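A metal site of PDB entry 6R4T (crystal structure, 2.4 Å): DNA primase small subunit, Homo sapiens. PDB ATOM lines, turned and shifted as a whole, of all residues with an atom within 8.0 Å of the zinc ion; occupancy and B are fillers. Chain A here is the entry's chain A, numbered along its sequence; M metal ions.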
ATOM      1  N   MET A 115      -8.875  22.872  26.830  1.00  0.00           N
ATOM      2  CA  MET A 115     -10.117  22.632  27.560  1.00  0.00           C
ATOM      3  C   MET A 115     -10.303  21.160  27.890  1.00  0.00           C
ATOM      4  O   MET A 115     -11.017  20.836  28.844  1.00  0.00           O
ATOM      5  CB  MET A 115     -11.307  23.134  26.745  1.00  0.00           C
ATOM      6  CG  MET A 115     -12.596  23.304  27.533  1.00  0.00           C
ATOM      7  SD  MET A 115     -12.730  24.901  28.362  1.00  0.00           S
ATOM      8  CE  MET A 115     -12.940  25.991  26.948  1.00  0.00           C
ATOM      9  N   ARG A 122     -16.037  19.321  33.710  1.00  0.00           N
ATOM     10  CA  ARG A 122     -16.992  19.827  32.733  1.00  0.00           C
ATOM     11  C   ARG A 122     -18.182  18.890  32.648  1.00  0.00           C
ATOM     12  O   ARG A 122     -18.010  17.667  32.528  1.00  0.00           O
ATOM     13  CB  ARG A 122     -16.342  19.966  31.348  1.00  0.00           C
ATOM     14  CG  ARG A 122     -15.742  21.325  31.057  1.00  0.00           C
ATOM     15  CD  ARG A 122     -15.538  21.510  29.552  1.00  0.00           C
ATOM     16  NE  ARG A 122     -14.706  20.452  28.982  1.00  0.00           N
ATOM     17  CZ  ARG A 122     -14.418  20.337  27.685  1.00  0.00           C
ATOM     18  NH1 ARG A 122     -14.893  21.212  26.816  1.00  0.00           N
ATOM     19  NH2 ARG A 122     -13.655  19.347  27.258  1.00  0.00           N
ATOM     20  N   ARG A 123     -19.389  19.458  32.700  1.00  0.00           N
ATOM     21  CA  ARG A 123     -20.621  18.695  32.566  1.00  0.00           C
ATOM     22  C   ARG A 123     -21.340  18.959  31.253  1.00  0.00           C
ATOM     23  O   ARG A 123     -22.375  18.338  30.986  1.00  0.00           O
ATOM     24  CB  ARG A 123     -21.580  19.005  33.731  1.00  0.00           C
ATOM     25  CG  ARG A 123     -21.036  18.656  35.108  1.00  0.00           C
ATOM     26  CD  ARG A 123     -22.048  18.927  36.238  1.00  0.00           C
ATOM     27  NE  ARG A 123     -23.075  17.888  36.330  1.00  0.00           N
ATOM     28  CZ  ARG A 123     -24.357  18.029  36.002  1.00  0.00           C
ATOM     29  NH1 ARG A 123     -24.827  19.193  35.557  1.00  0.00           N
ATOM     30  NH2 ARG A 123     -25.187  17.000  36.134  1.00  0.00           N
ATOM     31  N   CYS A 124     -20.810  19.858  30.418  1.00  0.00           N
ATOM     32  CA  CYS A 124     -21.457  20.249  29.167  1.00  0.00           C
ATOM     33  C   CYS A 124     -20.775  19.713  27.923  1.00  0.00           C
ATOM     34  O   CYS A 124     -21.458  19.323  26.974  1.00  0.00           O
ATOM     35  CB  CYS A 124     -21.532  21.777  29.079  1.00  0.00           C
ATOM     36  SG  CYS A 124     -19.922  22.595  29.276  1.00  0.00           S
ATOM     37  N   CYS A 125     -19.447  19.694  27.894  1.00  0.00           N
ATOM     38  CA  CYS A 125     -18.693  19.237  26.732  1.00  0.00           C
ATOM     39  C   CYS A 125     -17.696  18.175  27.165  1.00  0.00           C
ATOM     40  O   CYS A 125     -17.547  17.871  28.357  1.00  0.00           O
ATOM     41  CB  CYS A 125     -17.959  20.399  26.045  1.00  0.00           C
ATOM     42  SG  CYS A 125     -18.976  21.781  25.495  1.00  0.00           S
ATOM     43  N   SER A 126     -16.973  17.635  26.190  1.00  0.00           N
ATOM     44  CA  SER A 126     -15.906  16.674  26.448  1.00  0.00           C
ATOM     45  C   SER A 126     -14.951  16.687  25.259  1.00  0.00           C
ATOM     46  O   SER A 126     -15.295  17.165  24.172  1.00  0.00           O
ATOM     47  CB  SER A 126     -16.448  15.262  26.660  1.00  0.00           C
ATOM     48  OG  SER A 126     -17.079  14.769  25.490  1.00  0.00           O
ATOM     49  N   ASP A 129     -14.494  19.432  22.302  1.00  0.00           N
ATOM     50  CA  ASP A 129     -15.678  20.265  22.196  1.00  0.00           C
ATOM     51  C   ASP A 129     -15.606  21.448  23.148  1.00  0.00           C
ATOM     52  O   ASP A 129     -15.020  21.373  24.241  1.00  0.00           O
ATOM     53  CB  ASP A 129     -16.942  19.457  22.512  1.00  0.00           C
ATOM     54  CG  ASP A 129     -17.275  18.428  21.443  1.00  0.00           C
ATOM     55  OD1 ASP A 129     -16.935  18.664  20.263  1.00  0.00           O
ATOM     56  OD2 ASP A 129     -17.878  17.394  21.787  1.00  0.00           O
ATOM     57  N   ILE A 130     -16.176  22.583  22.721  1.00  0.00           N
ATOM     58  CA  ILE A 130     -16.306  23.763  23.559  1.00  0.00           C
ATOM     59  C   ILE A 130     -17.699  24.350  23.344  1.00  0.00           C
ATOM     60  O   ILE A 130     -18.369  24.090  22.348  1.00  0.00           O
ATOM     61  CB  ILE A 130     -15.218  24.824  23.286  1.00  0.00           C
ATOM     62  CG1 ILE A 130     -15.218  25.232  21.826  1.00  0.00           C
ATOM     63  CG2 ILE A 130     -13.854  24.284  23.711  1.00  0.00           C
ATOM     64  CD1 ILE A 130     -14.405  26.476  21.537  1.00  0.00           C
ATOM     65  N   CYS A 131     -18.125  25.155  24.313  1.00  0.00           N
ATOM     66  CA  CYS A 131     -19.430  25.814  24.238  1.00  0.00           C
ATOM     67  C   CYS A 131     -19.405  27.022  25.159  1.00  0.00           C
ATOM     68  O   CYS A 131     -18.508  27.143  26.014  1.00  0.00           O
ATOM     69  CB  CYS A 131     -20.556  24.865  24.653  1.00  0.00           C
ATOM     70  SG  CYS A 131     -20.664  24.632  26.429  1.00  0.00           S
ATOM     71  N   PRO A 132     -20.360  27.941  25.024  1.00  0.00           N
ATOM     72  CA  PRO A 132     -20.375  29.122  25.897  1.00  0.00           C
ATOM     73  C   PRO A 132     -20.474  28.811  27.376  1.00  0.00           C
ATOM     74  O   PRO A 132     -20.063  29.640  28.199  1.00  0.00           O
ATOM     75  CB  PRO A 132     -21.617  29.900  25.414  1.00  0.00           C
ATOM     76  CG  PRO A 132     -21.806  29.466  24.010  1.00  0.00           C
ATOM     77  CD  PRO A 132     -21.393  28.020  23.975  1.00  0.00           C
ATOM     78  N   LYS A 133     -21.007  27.648  27.760  1.00  0.00           N
ATOM     79  CA  LYS A 133     -21.151  27.350  29.181  1.00  0.00           C
ATOM     80  C   LYS A 133     -19.803  27.120  29.857  1.00  0.00           C
ATOM     81  O   LYS A 133     -19.624  27.484  31.026  1.00  0.00           O
ATOM     82  CB  LYS A 133     -22.036  26.121  29.401  1.00  0.00           C
ATOM     83  CG  LYS A 133     -23.528  26.372  29.398  1.00  0.00           C
ATOM     84  CD  LYS A 133     -24.264  25.120  29.876  1.00  0.00           C
ATOM     85  CE  LYS A 133     -25.724  25.392  30.184  1.00  0.00           C
ATOM     86  NZ  LYS A 133     -26.384  24.218  30.830  1.00  0.00           N
ATOM     87  N   CYS A 134     -18.850  26.528  29.146  1.00  0.00           N
ATOM     88  CA  CYS A 134     -17.565  26.187  29.739  1.00  0.00           C
ATOM     89  C   CYS A 134     -16.434  27.076  29.274  1.00  0.00           C
ATOM     90  O   CYS A 134     -15.337  26.983  29.825  1.00  0.00           O
ATOM     91  CB  CYS A 134     -17.200  24.717  29.429  1.00  0.00           C
ATOM     92  SG  CYS A 134     -17.140  24.308  27.678  1.00  0.00           S
ATOM     93  N   TRP A 135     -16.660  27.950  28.291  1.00  0.00           N
ATOM     94  CA  TRP A 135     -15.590  28.849  27.862  1.00  0.00           C
ATOM     95  C   TRP A 135     -15.168  29.796  28.976  1.00  0.00           C
ATOM     96  O   TRP A 135     -14.053  30.322  28.936  1.00  0.00           O
ATOM     97  CB  TRP A 135     -16.023  29.675  26.647  1.00  0.00           C
ATOM     98  CG  TRP A 135     -14.904  30.566  26.187  1.00  0.00           C
ATOM     99  CD1 TRP A 135     -14.802  31.907  26.369  1.00  0.00           C
ATOM    100  CD2 TRP A 135     -13.720  30.163  25.496  1.00  0.00           C
ATOM    101  NE1 TRP A 135     -13.634  32.379  25.825  1.00  0.00           N
ATOM    102  CE2 TRP A 135     -12.945  31.323  25.286  1.00  0.00           C
ATOM    103  CE3 TRP A 135     -13.229  28.932  25.027  1.00  0.00           C
ATOM    104  CZ2 TRP A 135     -11.726  31.290  24.625  1.00  0.00           C
ATOM    105  CZ3 TRP A 135     -12.015  28.907  24.370  1.00  0.00           C
ATOM    106  CH2 TRP A 135     -11.274  30.072  24.185  1.00  0.00           C
ATOM    107  N   LEU A 137     -14.140  29.036  31.712  1.00  0.00           N
ATOM    108  CA  LEU A 137     -12.886  28.511  32.257  1.00  0.00           C
ATOM    109  C   LEU A 137     -11.698  29.266  31.670  1.00  0.00           C
ATOM    110  O   LEU A 137     -10.860  29.800  32.403  1.00  0.00           O
ATOM    111  CB  LEU A 137     -12.783  27.005  31.990  1.00  0.00           C
ATOM    112  CG  LEU A 137     -13.753  26.106  32.755  1.00  0.00           C
ATOM    113  CD1 LEU A 137     -13.728  24.668  32.249  1.00  0.00           C
ATOM    114  CD2 LEU A 137     -13.459  26.141  34.257  1.00  0.00           C
ATOM    115  N   TYR A 229     -20.978  30.566  36.602  1.00  0.00           N
ATOM    116  CA  TYR A 229     -20.380  29.463  35.865  1.00  0.00           C
ATOM    117  C   TYR A 229     -20.664  28.121  36.538  1.00  0.00           C
ATOM    118  O   TYR A 229     -21.180  27.197  35.915  1.00  0.00           O
ATOM    119  CB  TYR A 229     -18.865  29.649  35.744  1.00  0.00           C
ATOM    120  CG  TYR A 229     -18.163  28.369  35.373  1.00  0.00           C
ATOM    121  CD1 TYR A 229     -18.179  27.889  34.069  1.00  0.00           C
ATOM    122  CD2 TYR A 229     -17.524  27.606  36.343  1.00  0.00           C
ATOM    123  CE1 TYR A 229     -17.554  26.697  33.737  1.00  0.00           C
ATOM    124  CE2 TYR A 229     -16.896  26.411  36.020  1.00  0.00           C
ATOM    125  CZ  TYR A 229     -16.924  25.965  34.708  1.00  0.00           C
ATOM    126  OH  TYR A 229     -16.312  24.775  34.382  1.00  0.00           O
ATOM    127  N   GLN A 234     -23.056  25.177  35.095  1.00  0.00           N
ATOM    128  CA  GLN A 234     -22.630  23.799  35.248  1.00  0.00           C
ATOM    129  C   GLN A 234     -23.522  23.037  36.218  1.00  0.00           C
ATOM    130  O   GLN A 234     -23.668  21.810  36.082  1.00  0.00           O
ATOM    131  CB  GLN A 234     -21.181  23.744  35.735  1.00  0.00           C
ATOM    132  CG  GLN A 234     -20.174  24.311  34.738  1.00  0.00           C
ATOM    133  CD  GLN A 234     -20.061  23.472  33.479  1.00  0.00           C
ATOM    134  OE1 GLN A 234     -19.955  22.251  33.538  1.00  0.00           O
ATOM    135  NE2 GLN A 234     -20.082  24.142  32.336  1.00  0.00           N
ATOM    136  N   PHE A 348     -16.894  31.581  19.176  1.00  0.00           N
ATOM    137  CA  PHE A 348     -17.848  31.155  18.152  1.00  0.00           C
ATOM    138  C   PHE A 348     -18.093  32.211  17.082  1.00  0.00           C
ATOM    139  O   PHE A 348     -18.719  31.899  16.067  1.00  0.00           O
ATOM    140  CB  PHE A 348     -19.129  30.710  18.843  1.00  0.00           C
ATOM    141  CG  PHE A 348     -18.876  29.792  20.001  1.00  0.00           C
ATOM    142  CD1 PHE A 348     -18.532  28.468  19.782  1.00  0.00           C
ATOM    143  CD2 PHE A 348     -18.925  30.259  21.303  1.00  0.00           C
ATOM    144  CE1 PHE A 348     -18.271  27.618  20.834  1.00  0.00           C
ATOM    145  CE2 PHE A 348     -18.666  29.415  22.369  1.00  0.00           C
ATOM    146  CZ  PHE A 348     -18.337  28.090  22.133  1.00  0.00           C
HETATM  147 ZN    ZN M   1     -19.285  23.177  27.211  1.00  0.00          ZN
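Of the 17 residues printed, 4 come within 4 Å of the zinc ion. The nearest printed residue that does not touch the zinc ion is Ile 130 (4.3 Å).
The side-chain sulfur (SG) of Cys 131 lies close to the backbone NH (N) of Lys 133 (3.3 Å). SG of Cys 124 sits close to NE2 of Gln 234 (3.4 Å).
SG of Cys 131 is bound to the zinc ion, 2.2 Å away. SG of Cys 125 binds the zinc ion, 2.2 Å away. The side-chain sulfur (SG) of Cys 124 is bound to the zinc ion, 2.2 Å away. SG of Cys 134 binds the zinc ion.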
